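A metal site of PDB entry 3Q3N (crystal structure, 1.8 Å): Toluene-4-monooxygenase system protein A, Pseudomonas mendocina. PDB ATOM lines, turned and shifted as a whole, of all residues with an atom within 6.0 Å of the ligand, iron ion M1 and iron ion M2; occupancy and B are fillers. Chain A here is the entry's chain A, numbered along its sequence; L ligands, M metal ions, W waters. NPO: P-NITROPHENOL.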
ATOM      1  N   ALA A  99       8.766  12.041  -6.341  1.00  0.00           N
ATOM      2  CA  ALA A  99       9.020  12.797  -5.109  1.00  0.00           C
ATOM      3  C   ALA A  99      10.176  13.787  -5.222  1.00  0.00           C
ATOM      4  O   ALA A  99      10.297  14.704  -4.398  1.00  0.00           O
ATOM      5  CB  ALA A  99       9.266  11.851  -3.944  1.00  0.00           C
ATOM      6  N   ILE A 100      11.024  13.584  -6.233  1.00  0.00           N
ATOM      7  CA  ILE A 100      12.312  14.288  -6.319  1.00  0.00           C
ATOM      8  C   ILE A 100      12.452  15.282  -7.481  1.00  0.00           C
ATOM      9  O   ILE A 100      12.904  16.410  -7.281  1.00  0.00           O
ATOM     10  CB  ILE A 100      13.466  13.260  -6.431  1.00  0.00           C
ATOM     11  CG1 ILE A 100      13.569  12.424  -5.151  1.00  0.00           C
ATOM     12  CG2 ILE A 100      14.796  13.955  -6.739  1.00  0.00           C
ATOM     13  CD1 ILE A 100      13.873  13.219  -3.905  1.00  0.00           C
ATOM     14  N   ALA A 101      12.071  14.877  -8.688  1.00  0.00           N
ATOM     15  CA  ALA A 101      12.394  15.666  -9.885  1.00  0.00           C
ATOM     16  C   ALA A 101      12.040  17.158  -9.813  1.00  0.00           C
ATOM     17  O   ALA A 101      12.866  18.033 -10.071  1.00  0.00           O
ATOM     18  CB  ALA A 101      11.816  15.015 -11.164  1.00  0.00           C
ATOM     19  N   VAL A 102      10.786  17.468  -9.496  1.00  0.00           N
ATOM     20  CA  VAL A 102      10.369  18.861  -9.492  1.00  0.00           C
ATOM     21  C   VAL A 102      10.820  19.595  -8.218  1.00  0.00           C
ATOM     22  O   VAL A 102      10.908  20.818  -8.205  1.00  0.00           O
ATOM     23  CB  VAL A 102       8.868  18.983  -9.830  1.00  0.00           C
ATOM     24  CG1 VAL A 102       8.367  20.424  -9.708  1.00  0.00           C
ATOM     25  CG2 VAL A 102       8.653  18.479 -11.251  1.00  0.00           C
ATOM     26  N   GLY A 103      11.143  18.824  -7.179  1.00  0.00           N
ATOM     27  CA  GLY A 103      11.734  19.375  -5.964  1.00  0.00           C
ATOM     28  C   GLY A 103      13.167  19.822  -6.212  1.00  0.00           C
ATOM     29  O   GLY A 103      13.604  20.860  -5.698  1.00  0.00           O
ATOM     30  N   GLU A 104      13.906  19.052  -7.001  1.00  0.00           N
ATOM     31  CA  GLU A 104      15.240  19.451  -7.447  1.00  0.00           C
ATOM     32  C   GLU A 104      15.127  20.795  -8.140  1.00  0.00           C
ATOM     33  O   GLU A 104      15.937  21.695  -7.930  1.00  0.00           O
ATOM     34  CB  GLU A 104      15.842  18.432  -8.429  1.00  0.00           C
ATOM     35  CG  GLU A 104      16.089  17.054  -7.843  1.00  0.00           C
ATOM     36  CD  GLU A 104      17.501  16.882  -7.344  1.00  0.00           C
ATOM     37  OE1 GLU A 104      17.983  15.734  -7.263  1.00  0.00           O
ATOM     38  OE2 GLU A 104      18.131  17.906  -7.031  1.00  0.00           O
ATOM     39  N   ALA A 106      12.801  23.046  -7.757  1.00  0.00           N
ATOM     40  CA  ALA A 106      12.539  24.002  -6.690  1.00  0.00           C
ATOM     41  C   ALA A 106      13.828  24.403  -5.963  1.00  0.00           C
ATOM     42  O   ALA A 106      13.998  25.543  -5.552  1.00  0.00           O
ATOM     43  CB  ALA A 106      11.496  23.444  -5.682  1.00  0.00           C
ATOM     44  N   ALA A 107      14.764  23.463  -5.799  1.00  0.00           N
ATOM     45  CA  ALA A 107      16.038  23.799  -5.145  1.00  0.00           C
ATOM     46  C   ALA A 107      16.849  24.868  -5.885  1.00  0.00           C
ATOM     47  O   ALA A 107      17.675  25.542  -5.278  1.00  0.00           O
ATOM     48  CB  ALA A 107      16.870  22.547  -4.914  1.00  0.00           C
ATOM     49  N   GLU A 111      18.916  28.061  -4.022  1.00  0.00           N
ATOM     50  CA  GLU A 111      20.247  28.534  -4.396  1.00  0.00           C
ATOM     51  C   GLU A 111      20.160  29.983  -4.893  1.00  0.00           C
ATOM     52  O   GLU A 111      20.978  30.823  -4.549  1.00  0.00           O
ATOM     53  CB  GLU A 111      20.853  27.608  -5.471  1.00  0.00           C
ATOM     54  CG  GLU A 111      21.145  26.178  -4.935  1.00  0.00           C
ATOM     55  CD  GLU A 111      22.394  26.106  -4.054  1.00  0.00           C
ATOM     56  OE1 GLU A 111      23.134  27.095  -4.014  1.00  0.00           O
ATOM     57  OE2 GLU A 111      22.626  25.065  -3.395  1.00  0.00           O
ATOM     58  N   ASP A 133      23.566  23.440 -10.797  1.00  0.00           N
ATOM     59  CA  ASP A 133      23.514  22.038 -10.387  1.00  0.00           C
ATOM     60  C   ASP A 133      22.075  21.564 -10.255  1.00  0.00           C
ATOM     61  O   ASP A 133      21.738  20.486 -10.714  1.00  0.00           O
ATOM     62  CB  ASP A 133      24.197  21.802  -9.034  1.00  0.00           C
ATOM     63  CG  ASP A 133      25.700  21.995  -9.082  1.00  0.00           C
ATOM     64  OD1 ASP A 133      26.309  21.934 -10.180  1.00  0.00           O
ATOM     65  OD2 ASP A 133      26.288  22.166  -7.987  1.00  0.00           O
ATOM     66  N   GLU A 134      21.237  22.321  -9.569  1.00  0.00           N
ATOM     67  CA  GLU A 134      19.869  21.842  -9.358  1.00  0.00           C
ATOM     68  C   GLU A 134      19.068  21.854 -10.650  1.00  0.00           C
ATOM     69  O   GLU A 134      18.182  21.030 -10.846  1.00  0.00           O
ATOM     70  CB  GLU A 134      19.149  22.643  -8.265  1.00  0.00           C
ATOM     71  CG  GLU A 134      19.869  22.678  -6.918  1.00  0.00           C
ATOM     72  CD  GLU A 134      20.046  21.301  -6.262  1.00  0.00           C
ATOM     73  OE1 GLU A 134      19.736  20.240  -6.865  1.00  0.00           O
ATOM     74  OE2 GLU A 134      20.526  21.292  -5.101  1.00  0.00           O
ATOM     75  N   HIS A 137      19.885  18.630 -12.116  1.00  0.00           N
ATOM     76  CA  HIS A 137      19.209  17.537 -11.423  1.00  0.00           C
ATOM     77  C   HIS A 137      17.740  17.414 -11.781  1.00  0.00           C
ATOM     78  O   HIS A 137      17.245  16.314 -11.965  1.00  0.00           O
ATOM     79  CB  HIS A 137      19.378  17.689  -9.907  1.00  0.00           C
ATOM     80  CG  HIS A 137      20.814  17.701  -9.480  1.00  0.00           C
ATOM     81  ND1 HIS A 137      21.219  18.046  -8.214  1.00  0.00           N
ATOM     82  CD2 HIS A 137      21.944  17.409 -10.171  1.00  0.00           C
ATOM     83  CE1 HIS A 137      22.542  17.983  -8.143  1.00  0.00           C
ATOM     84  NE2 HIS A 137      23.008  17.603  -9.316  1.00  0.00           N
ATOM     85  N   GLN A 141      16.211  14.283 -14.048  1.00  0.00           N
ATOM     86  CA  GLN A 141      15.216  13.421 -13.432  1.00  0.00           C
ATOM     87  C   GLN A 141      13.802  13.584 -13.991  1.00  0.00           C
ATOM     88  O   GLN A 141      12.892  12.883 -13.560  1.00  0.00           O
ATOM     89  CB  GLN A 141      15.296  13.524 -11.913  1.00  0.00           C
ATOM     90  CG  GLN A 141      16.606  12.914 -11.403  1.00  0.00           C
ATOM     91  CD  GLN A 141      16.879  13.235  -9.959  1.00  0.00           C
ATOM     92  OE1 GLN A 141      17.041  14.400  -9.587  1.00  0.00           O
ATOM     93  NE2 GLN A 141      16.951  12.204  -9.131  1.00  0.00           N
ATOM     94  N   TYR A 162       4.262  17.274  -8.033  1.00  0.00           N
ATOM     95  CA  TYR A 162       4.299  18.568  -7.344  1.00  0.00           C
ATOM     96  C   TYR A 162       3.185  19.491  -7.792  1.00  0.00           C
ATOM     97  O   TYR A 162       2.931  20.526  -7.173  1.00  0.00           O
ATOM     98  CB  TYR A 162       5.641  19.258  -7.525  1.00  0.00           C
ATOM     99  CG  TYR A 162       6.715  18.737  -6.600  1.00  0.00           C
ATOM    100  CD1 TYR A 162       7.109  17.407  -6.653  1.00  0.00           C
ATOM    101  CD2 TYR A 162       7.344  19.573  -5.680  1.00  0.00           C
ATOM    102  CE1 TYR A 162       8.098  16.908  -5.813  1.00  0.00           C
ATOM    103  CE2 TYR A 162       8.360  19.085  -4.835  1.00  0.00           C
ATOM    104  CZ  TYR A 162       8.721  17.754  -4.905  1.00  0.00           C
ATOM    105  OH  TYR A 162       9.722  17.253  -4.086  1.00  0.00           O
ATOM    106  N   PHE A 176       9.836  20.957   1.463  1.00  0.00           N
ATOM    107  CA  PHE A 176      10.762  21.713   0.624  1.00  0.00           C
ATOM    108  C   PHE A 176      10.449  23.208   0.596  1.00  0.00           C
ATOM    109  O   PHE A 176      11.356  24.045   0.533  1.00  0.00           O
ATOM    110  CB  PHE A 176      10.836  21.121  -0.785  1.00  0.00           C
ATOM    111  CG  PHE A 176      11.550  19.791  -0.834  1.00  0.00           C
ATOM    112  CD1 PHE A 176      12.776  19.637  -0.209  1.00  0.00           C
ATOM    113  CD2 PHE A 176      10.989  18.706  -1.481  1.00  0.00           C
ATOM    114  CE1 PHE A 176      13.445  18.428  -0.241  1.00  0.00           C
ATOM    115  CE2 PHE A 176      11.648  17.474  -1.526  1.00  0.00           C
ATOM    116  CZ  PHE A 176      12.869  17.333  -0.904  1.00  0.00           C
ATOM    117  N   ILE A 180      13.572  25.145   1.650  1.00  0.00           N
ATOM    118  CA  ILE A 180      14.195  25.601   0.416  1.00  0.00           C
ATOM    119  C   ILE A 180      13.692  26.960  -0.078  1.00  0.00           C
ATOM    120  O   ILE A 180      14.463  27.894  -0.245  1.00  0.00           O
ATOM    121  CB  ILE A 180      13.983  24.588  -0.727  1.00  0.00           C
ATOM    122  CG1 ILE A 180      14.579  23.226  -0.345  1.00  0.00           C
ATOM    123  CG2 ILE A 180      14.588  25.116  -2.013  1.00  0.00           C
ATOM    124  CD1 ILE A 180      14.633  22.234  -1.529  1.00  0.00           C
ATOM    125  N   LEU A 192      18.968  23.777   4.178  1.00  0.00           N
ATOM    126  CA  LEU A 192      19.125  23.048   2.922  1.00  0.00           C
ATOM    127  C   LEU A 192      20.555  22.538   2.737  1.00  0.00           C
ATOM    128  O   LEU A 192      20.790  21.323   2.724  1.00  0.00           O
ATOM    129  CB  LEU A 192      18.707  23.931   1.740  1.00  0.00           C
ATOM    130  CG  LEU A 192      18.994  23.349   0.351  1.00  0.00           C
ATOM    131  CD1 LEU A 192      18.256  22.032   0.152  1.00  0.00           C
ATOM    132  CD2 LEU A 192      18.616  24.355  -0.726  1.00  0.00           C
ATOM    133  N   PHE A 196      20.061  19.188   5.177  1.00  0.00           N
ATOM    134  CA  PHE A 196      19.489  18.256   4.229  1.00  0.00           C
ATOM    135  C   PHE A 196      20.539  17.686   3.275  1.00  0.00           C
ATOM    136  O   PHE A 196      20.589  16.474   3.057  1.00  0.00           O
ATOM    137  CB  PHE A 196      18.389  18.949   3.421  1.00  0.00           C
ATOM    138  CG  PHE A 196      17.582  18.021   2.556  1.00  0.00           C
ATOM    139  CD1 PHE A 196      16.835  16.999   3.128  1.00  0.00           C
ATOM    140  CD2 PHE A 196      17.548  18.181   1.181  1.00  0.00           C
ATOM    141  CE1 PHE A 196      16.083  16.150   2.328  1.00  0.00           C
ATOM    142  CE2 PHE A 196      16.805  17.328   0.381  1.00  0.00           C
ATOM    143  CZ  PHE A 196      16.060  16.309   0.962  1.00  0.00           C
ATOM    144  N   GLU A 197      21.377  18.550   2.714  1.00  0.00           N
ATOM    145  CA  GLU A 197      22.235  18.142   1.599  1.00  0.00           C
ATOM    146  C   GLU A 197      23.560  17.481   2.019  1.00  0.00           C
ATOM    147  O   GLU A 197      24.130  16.706   1.247  1.00  0.00           O
ATOM    148  CB  GLU A 197      22.508  19.308   0.634  1.00  0.00           C
ATOM    149  CG  GLU A 197      21.270  19.802  -0.130  1.00  0.00           C
ATOM    150  CD  GLU A 197      21.611  20.947  -1.095  1.00  0.00           C
ATOM    151  OE1 GLU A 197      22.491  21.775  -0.763  1.00  0.00           O
ATOM    152  OE2 GLU A 197      21.007  21.006  -2.187  1.00  0.00           O
ATOM    153  N   THR A 201      20.393  13.501   2.032  1.00  0.00           N
ATOM    154  CA  THR A 201      20.254  13.094   0.626  1.00  0.00           C
ATOM    155  C   THR A 201      21.117  11.885   0.303  1.00  0.00           C
ATOM    156  O   THR A 201      20.766  11.084  -0.569  1.00  0.00           O
ATOM    157  CB  THR A 201      20.534  14.222  -0.370  1.00  0.00           C
ATOM    158  OG1 THR A 201      21.847  14.754  -0.151  1.00  0.00           O
ATOM    159  CG2 THR A 201      19.496  15.339  -0.213  1.00  0.00           C
ATOM    160  N   PHE A 205      20.305   9.034  -2.623  1.00  0.00           N
ATOM    161  CA  PHE A 205      21.114   9.105  -3.834  1.00  0.00           C
ATOM    162  C   PHE A 205      22.353   8.204  -3.836  1.00  0.00           C
ATOM    163  O   PHE A 205      22.956   7.969  -4.878  1.00  0.00           O
ATOM    164  CB  PHE A 205      21.513  10.556  -4.132  1.00  0.00           C
ATOM    165  CG  PHE A 205      20.361  11.423  -4.560  1.00  0.00           C
ATOM    166  CD1 PHE A 205      19.494  11.958  -3.621  1.00  0.00           C
ATOM    167  CD2 PHE A 205      20.150  11.706  -5.896  1.00  0.00           C
ATOM    168  CE1 PHE A 205      18.422  12.767  -4.006  1.00  0.00           C
ATOM    169  CE2 PHE A 205      19.078  12.512  -6.289  1.00  0.00           C
ATOM    170  CZ  PHE A 205      18.215  13.031  -5.357  1.00  0.00           C
ATOM    171  N   ILE A 227      24.651  12.607  -9.806  1.00  0.00           N
ATOM    172  CA  ILE A 227      23.971  13.744  -9.213  1.00  0.00           C
ATOM    173  C   ILE A 227      24.595  14.123  -7.851  1.00  0.00           C
ATOM    174  O   ILE A 227      24.828  15.288  -7.549  1.00  0.00           O
ATOM    175  CB  ILE A 227      22.470  13.424  -9.062  1.00  0.00           C
ATOM    176  CG1 ILE A 227      21.765  13.566 -10.414  1.00  0.00           C
ATOM    177  CG2 ILE A 227      21.815  14.359  -8.028  1.00  0.00           C
ATOM    178  CD1 ILE A 227      20.293  13.123 -10.406  1.00  0.00           C
ATOM    179  N   ASP A 230      27.552  16.496  -7.491  1.00  0.00           N
ATOM    180  CA  ASP A 230      27.276  17.935  -7.462  1.00  0.00           C
ATOM    181  C   ASP A 230      26.876  18.371  -6.049  1.00  0.00           C
ATOM    182  O   ASP A 230      27.289  19.427  -5.548  1.00  0.00           O
ATOM    183  CB  ASP A 230      26.109  18.300  -8.392  1.00  0.00           C
ATOM    184  CG  ASP A 230      26.397  17.976  -9.841  1.00  0.00           C
ATOM    185  OD1 ASP A 230      27.534  18.162 -10.297  1.00  0.00           O
ATOM    186  OD2 ASP A 230      25.444  17.545 -10.525  1.00  0.00           O
ATOM    187  N   GLU A 231      26.014  17.558  -5.439  1.00  0.00           N
ATOM    188  CA  GLU A 231      25.539  17.823  -4.081  1.00  0.00           C
ATOM    189  C   GLU A 231      26.739  18.007  -3.171  1.00  0.00           C
ATOM    190  O   GLU A 231      26.785  18.933  -2.323  1.00  0.00           O
ATOM    191  CB  GLU A 231      24.692  16.643  -3.597  1.00  0.00           C
ATOM    192  CG  GLU A 231      24.124  16.787  -2.181  1.00  0.00           C
ATOM    193  CD  GLU A 231      22.775  17.446  -2.188  1.00  0.00           C
ATOM    194  OE1 GLU A 231      21.790  16.852  -1.721  1.00  0.00           O
ATOM    195  OE2 GLU A 231      22.708  18.577  -2.700  1.00  0.00           O
ATOM    196  N   HIS A 234      28.118  21.675  -3.716  1.00  0.00           N
ATOM    197  CA  HIS A 234      27.308  22.842  -3.311  1.00  0.00           C
ATOM    198  C   HIS A 234      26.771  22.742  -1.883  1.00  0.00           C
ATOM    199  O   HIS A 234      26.444  23.758  -1.283  1.00  0.00           O
ATOM    200  CB  HIS A 234      26.244  23.224  -4.350  1.00  0.00           C
ATOM    201  CG  HIS A 234      25.136  22.231  -4.535  1.00  0.00           C
ATOM    202  ND1 HIS A 234      24.831  21.676  -5.764  1.00  0.00           N
ATOM    203  CD2 HIS A 234      24.205  21.755  -3.668  1.00  0.00           C
ATOM    204  CE1 HIS A 234      23.777  20.886  -5.639  1.00  0.00           C
ATOM    205  NE2 HIS A 234      23.384  20.912  -4.380  1.00  0.00           N
HETATM  206  C1  NPO L   1      15.838  17.806  -3.647  1.00  0.00           C
HETATM  207  C2  NPO L   1      16.733  16.762  -3.793  1.00  0.00           C
HETATM  208  C3  NPO L   1      18.090  17.022  -3.849  1.00  0.00           C
HETATM  209  C4  NPO L   1      18.552  18.323  -3.768  1.00  0.00           C
HETATM  210  C5  NPO L   1      17.657  19.368  -3.622  1.00  0.00           C
HETATM  211  C6  NPO L   1      16.300  19.108  -3.566  1.00  0.00           C
HETATM  212  OH  NPO L   1      19.909  18.580  -3.833  1.00  0.00           O
HETATM  213  N1  NPO L   1      14.436  17.546  -3.587  1.00  0.00           N
HETATM  214  O2  NPO L   1      13.599  18.525  -3.446  1.00  0.00           O
HETATM  215  O3  NPO L   1      14.022  16.400  -3.658  1.00  0.00           O
HETATM  216 FE    FE M   1      20.057  18.223  -6.366  1.00  0.00          FE
HETATM  217 FE    FE M   2      21.490  19.754  -3.906  1.00  0.00          FE
HETATM  218  O   HOH W   1      20.212  16.196  -5.922  1.00  0.00           O
HETATM  219  O   HOH W   2      21.027  15.225  -3.747  1.00  0.00           O
HETATM  220  O   HOH W   3      21.944  18.484  -5.458  1.00  0.00           O
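Iron ion M1 is bound by OE2 of Glu 104 (2.1 Å), water W1 (2.1 Å), OE1 of Glu 134 (2.1 Å), water W3 (2.1 Å), ND1 of His 137 (2.2 Å) and OH of the ligand (2.6 Å). Iron ion M1 has six donor atoms within binding distance.
O of Gly 103 sits close to O2 of the ligand (3.2 Å). Ile 100 touches the ligand (CD1 to O3, 3.2 Å). Ala 107 touches the ligand (CB to C5, 3.5 Å). Phe 176 touches the ligand. Eight residues have an atom within 4 Å of the ligand: Ile 100, Gly 103, Glu 104, Ala 107, Glu 134, Phe 176, Glu 197 and Glu 231. The nearest printed residue that does not touch the ligand is Ile 180 (4.1 Å).
The nearest printed residue that does not touch iron ion M1 is Glu 231 (4.5 Å).
OE1 of Glu 104 sits close to OE1 of Gln 141 (2.8 Å). The side-chain carboxylate of Glu 231 is in hydrogen-bond range of the side-chain hydroxyl of Thr 201. The side-chain hydroxyl of Thr 201 sits at hydrogen-bond distance from the backbone carbonyl oxygen of Glu 197. The backbone carbonyl oxygen of Leu 192 is in hydrogen-bond range of the backbone NH of Glu 197 (2.8 Å). O of Ile 227 sits at hydrogen-bond distance from NE2 of His 137. A ring nitrogen (NE2) of His 137 is in hydrogen-bond range of the side-chain carboxylate (OD2) of Asp 230, at 2.7 Å. OD2 of Asp 133 sits at hydrogen-bond distance from ND1 of His 234 (2.7 Å). A ring nitrogen (ND1) of His 234 sits at hydrogen-bond distance from the backbone carbonyl oxygen (O) of Asp 230 (3.3 Å).
Iron ion M2 is bound by OH of the ligand (2.0 Å), water W3 (2.1 Å), OE2 of Glu 231 (2.1 Å), OE2 of Glu 134 (2.2 Å), OE2 of Glu 197 (2.2 Å) and NE2 of His 234 (2.3 Å). Iron ion M2 has six donor atoms within binding distance.
The nearest printed residue that does not touch iron ion M2 is His 137 (4.6 Å).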
